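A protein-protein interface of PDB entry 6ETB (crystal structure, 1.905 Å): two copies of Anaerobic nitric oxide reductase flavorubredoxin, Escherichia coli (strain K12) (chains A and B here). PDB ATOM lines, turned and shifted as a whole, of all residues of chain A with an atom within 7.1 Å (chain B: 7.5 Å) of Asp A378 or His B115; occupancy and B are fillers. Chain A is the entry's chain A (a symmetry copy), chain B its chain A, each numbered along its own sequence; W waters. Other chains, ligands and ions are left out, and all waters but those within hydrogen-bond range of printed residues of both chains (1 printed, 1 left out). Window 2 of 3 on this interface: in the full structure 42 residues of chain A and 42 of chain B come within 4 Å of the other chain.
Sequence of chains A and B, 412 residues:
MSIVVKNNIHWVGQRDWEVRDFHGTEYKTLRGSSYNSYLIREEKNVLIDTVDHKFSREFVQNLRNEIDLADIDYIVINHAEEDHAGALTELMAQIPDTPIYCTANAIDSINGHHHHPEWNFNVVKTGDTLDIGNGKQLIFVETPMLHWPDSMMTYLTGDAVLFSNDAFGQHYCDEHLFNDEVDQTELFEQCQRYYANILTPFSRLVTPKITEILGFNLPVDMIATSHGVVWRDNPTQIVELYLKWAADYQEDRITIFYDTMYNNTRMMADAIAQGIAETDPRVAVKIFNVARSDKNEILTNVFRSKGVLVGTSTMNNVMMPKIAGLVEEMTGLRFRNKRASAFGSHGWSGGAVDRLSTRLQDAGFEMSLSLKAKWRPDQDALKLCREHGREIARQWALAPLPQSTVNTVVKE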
ATOM      1  N   MET A 267     -15.334 -22.487 -30.014  1.00  0.00           N
ATOM      2  CA  MET A 267     -15.498 -23.904 -29.716  1.00  0.00           C
ATOM      3  C   MET A 267     -16.971 -24.291 -29.748  1.00  0.00           C
ATOM      4  O   MET A 267     -17.330 -25.372 -30.214  1.00  0.00           O
ATOM      5  CB  MET A 267     -14.889 -24.239 -28.352  1.00  0.00           C
ATOM      6  CG  MET A 267     -13.377 -24.101 -28.302  1.00  0.00           C
ATOM      7  SD  MET A 267     -12.707 -24.369 -26.650  1.00  0.00           S
ATOM      8  CE  MET A 267     -13.214 -26.059 -26.346  1.00  0.00           C
ATOM      9  N   LYS A 374     -20.392 -21.644 -19.831  1.00  0.00           N
ATOM     10  CA  LYS A 374     -19.519 -20.908 -18.923  1.00  0.00           C
ATOM     11  C   LYS A 374     -18.049 -21.225 -19.188  1.00  0.00           C
ATOM     12  O   LYS A 374     -17.654 -22.393 -19.207  1.00  0.00           O
ATOM     13  CB  LYS A 374     -19.882 -21.225 -17.470  1.00  0.00           C
ATOM     14  CG  LYS A 374     -19.339 -20.235 -16.455  1.00  0.00           C
ATOM     15  CD  LYS A 374     -19.807 -20.584 -15.050  1.00  0.00           C
ATOM     16  CE  LYS A 374     -19.314 -19.570 -14.033  1.00  0.00           C
ATOM     17  NZ  LYS A 374     -19.738 -19.924 -12.650  1.00  0.00           N
ATOM     18  N   TRP A 375     -17.254 -20.175 -19.386  1.00  0.00           N
ATOM     19  CA  TRP A 375     -15.825 -20.297 -19.676  1.00  0.00           C
ATOM     20  C   TRP A 375     -15.563 -21.197 -20.880  1.00  0.00           C
ATOM     21  O   TRP A 375     -16.292 -21.153 -21.871  1.00  0.00           O
ATOM     22  CB  TRP A 375     -15.065 -20.830 -18.456  1.00  0.00           C
ATOM     23  CG  TRP A 375     -15.222 -19.997 -17.220  1.00  0.00           C
ATOM     24  CD1 TRP A 375     -15.800 -20.377 -16.044  1.00  0.00           C
ATOM     25  CD2 TRP A 375     -14.803 -18.640 -17.039  1.00  0.00           C
ATOM     26  NE1 TRP A 375     -15.758 -19.344 -15.140  1.00  0.00           N
ATOM     27  CE2 TRP A 375     -15.152 -18.265 -15.727  1.00  0.00           C
ATOM     28  CE3 TRP A 375     -14.164 -17.706 -17.861  1.00  0.00           C
ATOM     29  CZ2 TRP A 375     -14.884 -16.997 -15.218  1.00  0.00           C
ATOM     30  CZ3 TRP A 375     -13.897 -16.448 -17.352  1.00  0.00           C
ATOM     31  CH2 TRP A 375     -14.257 -16.106 -16.044  1.00  0.00           C
ATOM     32  N   ARG A 376     -14.519 -22.014 -20.783  1.00  0.00           N
ATOM     33  CA  ARG A 376     -14.177 -22.952 -21.843  1.00  0.00           C
ATOM     34  C   ARG A 376     -15.018 -24.219 -21.729  1.00  0.00           C
ATOM     35  O   ARG A 376     -14.993 -24.893 -20.699  1.00  0.00           O
ATOM     36  CB  ARG A 376     -12.688 -23.301 -21.793  1.00  0.00           C
ATOM     37  CG  ARG A 376     -12.241 -24.294 -22.856  1.00  0.00           C
ATOM     38  CD  ARG A 376     -10.744 -24.553 -22.778  1.00  0.00           C
ATOM     39  NE  ARG A 376      -9.960 -23.352 -23.055  1.00  0.00           N
ATOM     40  CZ  ARG A 376      -9.472 -23.038 -24.251  1.00  0.00           C
ATOM     41  NH1 ARG A 376      -9.686 -23.837 -25.287  1.00  0.00           N
ATOM     42  NH2 ARG A 376      -8.769 -21.925 -24.411  1.00  0.00           N
ATOM     43  N   PRO A 377     -15.773 -24.542 -22.788  1.00  0.00           N
ATOM     44  CA  PRO A 377     -16.628 -25.735 -22.800  1.00  0.00           C
ATOM     45  C   PRO A 377     -15.823 -27.027 -22.711  1.00  0.00           C
ATOM     46  O   PRO A 377     -14.953 -27.261 -23.550  1.00  0.00           O
ATOM     47  CB  PRO A 377     -17.351 -25.639 -24.149  1.00  0.00           C
ATOM     48  CG  PRO A 377     -17.233 -24.200 -24.552  1.00  0.00           C
ATOM     49  CD  PRO A 377     -15.907 -23.758 -24.027  1.00  0.00           C
ATOM     50  N   ASP A 378     -16.107 -27.854 -21.709  1.00  0.00           N
ATOM     51  CA  ASP A 378     -15.446 -29.148 -21.600  1.00  0.00           C
ATOM     52  C   ASP A 378     -16.138 -30.161 -22.506  1.00  0.00           C
ATOM     53  O   ASP A 378     -16.966 -29.789 -23.336  1.00  0.00           O
ATOM     54  CB  ASP A 378     -15.425 -29.638 -20.145  1.00  0.00           C
ATOM     55  CG  ASP A 378     -16.797 -29.617 -19.487  1.00  0.00           C
ATOM     56  OD1 ASP A 378     -17.817 -29.799 -20.183  1.00  0.00           O
ATOM     57  OD2 ASP A 378     -16.852 -29.415 -18.255  1.00  0.00           O
ATOM     58  N   GLN A 379     -15.801 -31.435 -22.339  1.00  0.00           N
ATOM     59  CA  GLN A 379     -16.362 -32.487 -23.181  1.00  0.00           C
ATOM     60  C   GLN A 379     -17.877 -32.579 -23.036  1.00  0.00           C
ATOM     61  O   GLN A 379     -18.589 -32.753 -24.023  1.00  0.00           O
ATOM     62  CB  GLN A 379     -15.719 -33.835 -22.851  1.00  0.00           C
ATOM     63  CG  GLN A 379     -14.233 -33.894 -23.159  1.00  0.00           C
ATOM     64  CD  GLN A 379     -13.926 -33.567 -24.607  1.00  0.00           C
ATOM     65  OE1 GLN A 379     -14.370 -34.263 -25.520  1.00  0.00           O
ATOM     66  NE2 GLN A 379     -13.166 -32.499 -24.824  1.00  0.00           N
ATOM     67  N   ASP A 380     -18.363 -32.454 -21.807  1.00  0.00           N
ATOM     68  CA  ASP A 380     -19.797 -32.509 -21.542  1.00  0.00           C
ATOM     69  C   ASP A 380     -20.504 -31.268 -22.078  1.00  0.00           C
ATOM     70  O   ASP A 380     -21.619 -31.352 -22.592  1.00  0.00           O
ATOM     71  CB  ASP A 380     -20.063 -32.662 -20.045  1.00  0.00           C
ATOM     72  CG  ASP A 380     -19.572 -33.989 -19.499  1.00  0.00           C
ATOM     73  OD1 ASP A 380     -19.614 -34.993 -20.241  1.00  0.00           O
ATOM     74  OD2 ASP A 380     -19.144 -34.027 -18.326  1.00  0.00           O
ATOM     75  N   ALA A 381     -19.854 -30.115 -21.951  1.00  0.00           N
ATOM     76  CA  ALA A 381     -20.425 -28.862 -22.433  1.00  0.00           C
ATOM     77  C   ALA A 381     -20.504 -28.855 -23.955  1.00  0.00           C
ATOM     78  O   ALA A 381     -21.480 -28.373 -24.531  1.00  0.00           O
ATOM     79  CB  ALA A 381     -19.612 -27.679 -21.938  1.00  0.00           C
ATOM     80  N   LEU A 382     -19.477 -29.397 -24.601  1.00  0.00           N
ATOM     81  CA  LEU A 382     -19.449 -29.474 -26.058  1.00  0.00           C
ATOM     82  C   LEU A 382     -20.537 -30.410 -26.574  1.00  0.00           C
ATOM     83  O   LEU A 382     -21.017 -30.255 -27.697  1.00  0.00           O
ATOM     84  CB  LEU A 382     -18.077 -29.936 -26.552  1.00  0.00           C
ATOM     85  CG  LEU A 382     -16.944 -28.908 -26.481  1.00  0.00           C
ATOM     86  CD1 LEU A 382     -15.645 -29.504 -26.998  1.00  0.00           C
ATOM     87  CD2 LEU A 382     -17.308 -27.655 -27.260  1.00  0.00           C
ATOM     88  N   LYS A 383     -20.920 -31.380 -25.749  1.00  0.00           N
ATOM     89  CA  LYS A 383     -22.019 -32.277 -26.082  1.00  0.00           C
ATOM     90  C   LYS A 383     -23.332 -31.507 -26.152  1.00  0.00           C
ATOM     91  O   LYS A 383     -24.151 -31.741 -27.038  1.00  0.00           O
ATOM     92  CB  LYS A 383     -22.131 -33.411 -25.060  1.00  0.00           C
ATOM     93  CG  LYS A 383     -21.013 -34.436 -25.135  1.00  0.00           C
ATOM     94  CD  LYS A 383     -21.198 -35.531 -24.097  1.00  0.00           C
ATOM     95  CE  LYS A 383     -20.023 -36.495 -24.094  1.00  0.00           C
ATOM     96  NZ  LYS A 383     -19.859 -37.172 -25.411  1.00  0.00           N
ATOM     97  N   LEU A 384     -23.525 -30.590 -25.208  1.00  0.00           N
ATOM     98  CA  LEU A 384     -24.725 -29.761 -25.181  1.00  0.00           C
ATOM     99  C   LEU A 384     -24.763 -28.819 -26.381  1.00  0.00           C
ATOM    100  O   LEU A 384     -25.824 -28.577 -26.955  1.00  0.00           O
ATOM    101  CB  LEU A 384     -24.801 -28.964 -23.877  1.00  0.00           C
ATOM    102  CG  LEU A 384     -25.033 -29.776 -22.599  1.00  0.00           C
ATOM    103  CD1 LEU A 384     -25.078 -28.865 -21.382  1.00  0.00           C
ATOM    104  CD2 LEU A 384     -26.309 -30.599 -22.706  1.00  0.00           C
ATOM    105  N   CYS A 385     -23.601 -28.288 -26.751  1.00  0.00           N
ATOM    106  CA  CYS A 385     -23.488 -27.440 -27.935  1.00  0.00           C
ATOM    107  C   CYS A 385     -23.790 -28.244 -29.193  1.00  0.00           C
ATOM    108  O   CYS A 385     -24.513 -27.789 -30.079  1.00  0.00           O
ATOM    109  CB  CYS A 385     -22.095 -26.818 -28.033  1.00  0.00           C
ATOM    110  SG  CYS A 385     -21.653 -25.718 -26.674  1.00  0.00           S
ATOM    111  N   THR B  89      -1.355 -24.975 -17.036  1.00  0.00           N
ATOM    112  CA  THR B  89      -1.533 -26.394 -17.337  1.00  0.00           C
ATOM    113  C   THR B  89      -0.203 -27.074 -17.650  1.00  0.00           C
ATOM    114  O   THR B  89       0.076 -28.168 -17.158  1.00  0.00           O
ATOM    115  CB  THR B  89      -2.500 -26.600 -18.523  1.00  0.00           C
ATOM    116  OG1 THR B  89      -3.811 -26.153 -18.156  1.00  0.00           O
ATOM    117  CG2 THR B  89      -2.569 -28.068 -18.914  1.00  0.00           C
ATOM    118  N   SER B 109     -12.780 -20.042 -12.024  1.00  0.00           N
ATOM    119  CA  SER B 109     -12.199 -19.563 -13.278  1.00  0.00           C
ATOM    120  C   SER B 109     -11.044 -20.446 -13.750  1.00  0.00           C
ATOM    121  O   SER B 109     -10.873 -20.660 -14.950  1.00  0.00           O
ATOM    122  CB  SER B 109     -11.726 -18.114 -13.135  1.00  0.00           C
ATOM    123  OG  SER B 109     -10.671 -18.001 -12.197  1.00  0.00           O
ATOM    124  N   ILE B 110     -10.253 -20.956 -12.809  1.00  0.00           N
ATOM    125  CA  ILE B 110      -9.162 -21.869 -13.143  1.00  0.00           C
ATOM    126  C   ILE B 110      -9.713 -23.178 -13.694  1.00  0.00           C
ATOM    127  O   ILE B 110      -9.322 -23.619 -14.775  1.00  0.00           O
ATOM    128  CB  ILE B 110      -8.265 -22.165 -11.924  1.00  0.00           C
ATOM    129  CG1 ILE B 110      -7.435 -20.933 -11.561  1.00  0.00           C
ATOM    130  CG2 ILE B 110      -7.340 -23.336 -12.210  1.00  0.00           C
ATOM    131  CD1 ILE B 110      -6.629 -21.092 -10.284  1.00  0.00           C
ATOM    132  N   ASN B 111     -10.629 -23.793 -12.950  1.00  0.00           N
ATOM    133  CA  ASN B 111     -11.275 -25.023 -13.393  1.00  0.00           C
ATOM    134  C   ASN B 111     -12.128 -24.792 -14.637  1.00  0.00           C
ATOM    135  O   ASN B 111     -12.408 -25.722 -15.392  1.00  0.00           O
ATOM    136  CB  ASN B 111     -12.139 -25.617 -12.277  1.00  0.00           C
ATOM    137  CG  ASN B 111     -11.318 -26.132 -11.109  1.00  0.00           C
ATOM    138  OD1 ASN B 111     -10.160 -26.522 -11.269  1.00  0.00           O
ATOM    139  ND2 ASN B 111     -11.921 -26.146  -9.926  1.00  0.00           N
ATOM    140  N   GLY B 112     -12.543 -23.546 -14.837  1.00  0.00           N
ATOM    141  CA  GLY B 112     -13.349 -23.183 -15.989  1.00  0.00           C
ATOM    142  C   GLY B 112     -12.612 -23.299 -17.309  1.00  0.00           C
ATOM    143  O   GLY B 112     -13.218 -23.592 -18.339  1.00  0.00           O
ATOM    144  N   HIS B 113     -11.300 -23.087 -17.282  1.00  0.00           N
ATOM    145  CA  HIS B 113     -10.503 -23.143 -18.502  1.00  0.00           C
ATOM    146  C   HIS B 113      -9.633 -24.397 -18.573  1.00  0.00           C
ATOM    147  O   HIS B 113      -9.520 -25.021 -19.629  1.00  0.00           O
ATOM    148  CB  HIS B 113      -9.623 -21.897 -18.620  1.00  0.00           C
ATOM    149  CG  HIS B 113      -8.921 -21.778 -19.938  1.00  0.00           C
ATOM    150  ND1 HIS B 113      -7.760 -22.463 -20.228  1.00  0.00           N
ATOM    151  CD2 HIS B 113      -9.216 -21.054 -21.043  1.00  0.00           C
ATOM    152  CE1 HIS B 113      -7.372 -22.166 -21.454  1.00  0.00           C
ATOM    153  NE2 HIS B 113      -8.236 -21.313 -21.971  1.00  0.00           N
ATOM    154  N   HIS B 114      -9.019 -24.763 -17.453  1.00  0.00           N
ATOM    155  CA  HIS B 114      -8.093 -25.891 -17.425  1.00  0.00           C
ATOM    156  C   HIS B 114      -8.767 -27.248 -17.246  1.00  0.00           C
ATOM    157  O   HIS B 114      -8.247 -28.262 -17.710  1.00  0.00           O
ATOM    158  CB  HIS B 114      -7.064 -25.683 -16.312  1.00  0.00           C
ATOM    159  CG  HIS B 114      -6.261 -24.429 -16.464  1.00  0.00           C
ATOM    160  ND1 HIS B 114      -5.118 -24.367 -17.232  1.00  0.00           N
ATOM    161  CD2 HIS B 114      -6.439 -23.189 -15.953  1.00  0.00           C
ATOM    162  CE1 HIS B 114      -4.625 -23.142 -17.184  1.00  0.00           C
ATOM    163  NE2 HIS B 114      -5.408 -22.408 -16.414  1.00  0.00           N
ATOM    164  N   HIS B 115      -9.913 -27.258 -16.569  1.00  0.00           N
ATOM    165  CA  HIS B 115     -10.661 -28.485 -16.300  1.00  0.00           C
ATOM    166  C   HIS B 115      -9.846 -29.472 -15.470  1.00  0.00           C
ATOM    167  O   HIS B 115      -9.900 -30.679 -15.704  1.00  0.00           O
ATOM    168  CB  HIS B 115     -11.106 -29.161 -17.601  1.00  0.00           C
ATOM    169  CG  HIS B 115     -11.850 -28.256 -18.532  1.00  0.00           C
ATOM    170  ND1 HIS B 115     -12.409 -27.065 -18.125  1.00  0.00           N
ATOM    171  CD2 HIS B 115     -12.125 -28.371 -19.853  1.00  0.00           C
ATOM    172  CE1 HIS B 115     -12.997 -26.484 -19.155  1.00  0.00           C
ATOM    173  NE2 HIS B 115     -12.840 -27.255 -20.215  1.00  0.00           N
ATOM    174  N   HIS B 116      -9.089 -28.956 -14.507  1.00  0.00           N
ATOM    175  CA  HIS B 116      -8.323 -29.806 -13.600  1.00  0.00           C
ATOM    176  C   HIS B 116      -8.658 -29.523 -12.138  1.00  0.00           C
ATOM    177  O   HIS B 116      -7.854 -28.932 -11.418  1.00  0.00           O
ATOM    178  CB  HIS B 116      -6.820 -29.621 -13.821  1.00  0.00           C
ATOM    179  CG  HIS B 116      -6.312 -30.229 -15.091  1.00  0.00           C
ATOM    180  ND1 HIS B 116      -6.011 -31.569 -15.206  1.00  0.00           N
ATOM    181  CD2 HIS B 116      -6.034 -29.677 -16.297  1.00  0.00           C
ATOM    182  CE1 HIS B 116      -5.580 -31.819 -16.430  1.00  0.00           C
ATOM    183  NE2 HIS B 116      -5.585 -30.687 -17.112  1.00  0.00           N
ATOM    184  N   PRO B 117      -9.849 -29.952 -11.691  1.00  0.00           N
ATOM    185  CA  PRO B 117     -10.270 -29.688 -10.311  1.00  0.00           C
ATOM    186  C   PRO B 117      -9.499 -30.521  -9.289  1.00  0.00           C
ATOM    187  O   PRO B 117      -9.615 -30.275  -8.089  1.00  0.00           O
ATOM    188  CB  PRO B 117     -11.751 -30.070 -10.321  1.00  0.00           C
ATOM    189  CG  PRO B 117     -11.850 -31.118 -11.373  1.00  0.00           C
ATOM    190  CD  PRO B 117     -10.858 -30.727 -12.437  1.00  0.00           C
ATOM    191  N   GLU B 118      -8.717 -31.488  -9.761  1.00  0.00           N
ATOM    192  CA  GLU B 118      -7.962 -32.353  -8.863  1.00  0.00           C
ATOM    193  C   GLU B 118      -6.753 -31.632  -8.273  1.00  0.00           C
ATOM    194  O   GLU B 118      -6.113 -32.136  -7.351  1.00  0.00           O
ATOM    195  CB  GLU B 118      -7.509 -33.625  -9.586  1.00  0.00           C
ATOM    196  CG  GLU B 118      -6.350 -33.430 -10.553  1.00  0.00           C
ATOM    197  CD  GLU B 118      -6.783 -32.867 -11.891  1.00  0.00           C
ATOM    198  OE1 GLU B 118      -8.002 -32.709 -12.110  1.00  0.00           O
ATOM    199  OE2 GLU B 118      -5.900 -32.588 -12.728  1.00  0.00           O
ATOM    200  N   TRP B 119      -6.441 -30.455  -8.810  1.00  0.00           N
ATOM    201  CA  TRP B 119      -5.358 -29.632  -8.278  1.00  0.00           C
ATOM    202  C   TRP B 119      -5.647 -29.221  -6.836  1.00  0.00           C
ATOM    203  O   TRP B 119      -6.804 -29.148  -6.425  1.00  0.00           O
ATOM    204  CB  TRP B 119      -5.146 -28.392  -9.148  1.00  0.00           C
ATOM    205  CG  TRP B 119      -4.536 -28.687 -10.485  1.00  0.00           C
ATOM    206  CD1 TRP B 119      -3.898 -29.834 -10.863  1.00  0.00           C
ATOM    207  CD2 TRP B 119      -4.510 -27.820 -11.626  1.00  0.00           C
ATOM    208  NE1 TRP B 119      -3.475 -29.733 -12.166  1.00  0.00           N
ATOM    209  CE2 TRP B 119      -3.837 -28.507 -12.657  1.00  0.00           C
ATOM    210  CE3 TRP B 119      -4.988 -26.531 -11.874  1.00  0.00           C
ATOM    211  CZ2 TRP B 119      -3.636 -27.947 -13.918  1.00  0.00           C
ATOM    212  CZ3 TRP B 119      -4.784 -25.976 -13.126  1.00  0.00           C
ATOM    213  CH2 TRP B 119      -4.113 -26.684 -14.131  1.00  0.00           C
HETATM  214  O   HOH W   1     -14.894 -27.540 -16.912  1.00  0.00           O
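A ring nitrogen (NE2) of His B113 is in hydrogen-bond range of the guanidinium group (NH2) of Arg A376, at 2.6 Å.
A ring nitrogen (NE2) of His B115 sits close to the backbone carbonyl oxygen (O) of Arg A376, 3.2 Å away.
O of Gly B112 lies within hydrogen-bond range of N of Arg A376, at 3.2 Å.
The backbone NH of Ala A381 is in hydrogen-bond range of the side-chain carboxylate of Asp A378 (2.7 Å).
N of Asp A380 is in hydrogen-bond range of OD1 of Asp A378 (3.2 Å).
The backbone carbonyl oxygen (O) of Asn B111 is in hydrogen-bond range of a ring nitrogen (ND1) of His B115, 3.0 Å away.
The side-chain sulfur of Met A267 sits at hydrogen-bond distance from the guanidinium group of Arg A376, at 3.4 Å.
Among the printed residues, pairs that only touch across the chains: Trp A375 with Ser B109 (3.9 Å), Trp A375 with Gly B112 (3.3 Å), Pro A377 with His B115 (3.9 Å) and Asp A378 with His B115 (3.5 Å).
Of chain B, only His B115 comes within 4 Å of Asp A378.
Of the printed residues of chain A, His B115 touches Arg A376 (3.0 Å), Pro A377 (3.9 Å) and Asp A378 (3.5 Å).
Printed residues of chain B within 4 Å of Pro A377: His B115.
Of the printed residues of chain B, Trp A375 touches Ser B109 (3.9 Å) and Gly B112 (3.3 Å).
Printed residues of chain A within 4 Å of Gly B112: Trp A375 and Arg A376.
Of the printed residues of chain B, Arg A376 touches Gly B112 (3.2 Å), His B113 (2.6 Å) and His B115 (3.0 Å).
Hydrophobic or aromatic side chains of chain B within 4 Å of the printed part of chain A: His B113 and His B115.
Of the 13 printed residues of chain A, 4 touch a printed residue of chain B.
No position is printed for both chains.
Of the 7 pairs that touch across the chains among the printed residues, none has its exchanged pair printed and touching as well.
Water W1 lies within hydrogen-bond range of ND1 of His B115 (2.8 Å), OD2 of Asp A378 (3.0 Å) and O of Asn B111 (3.4 Å).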
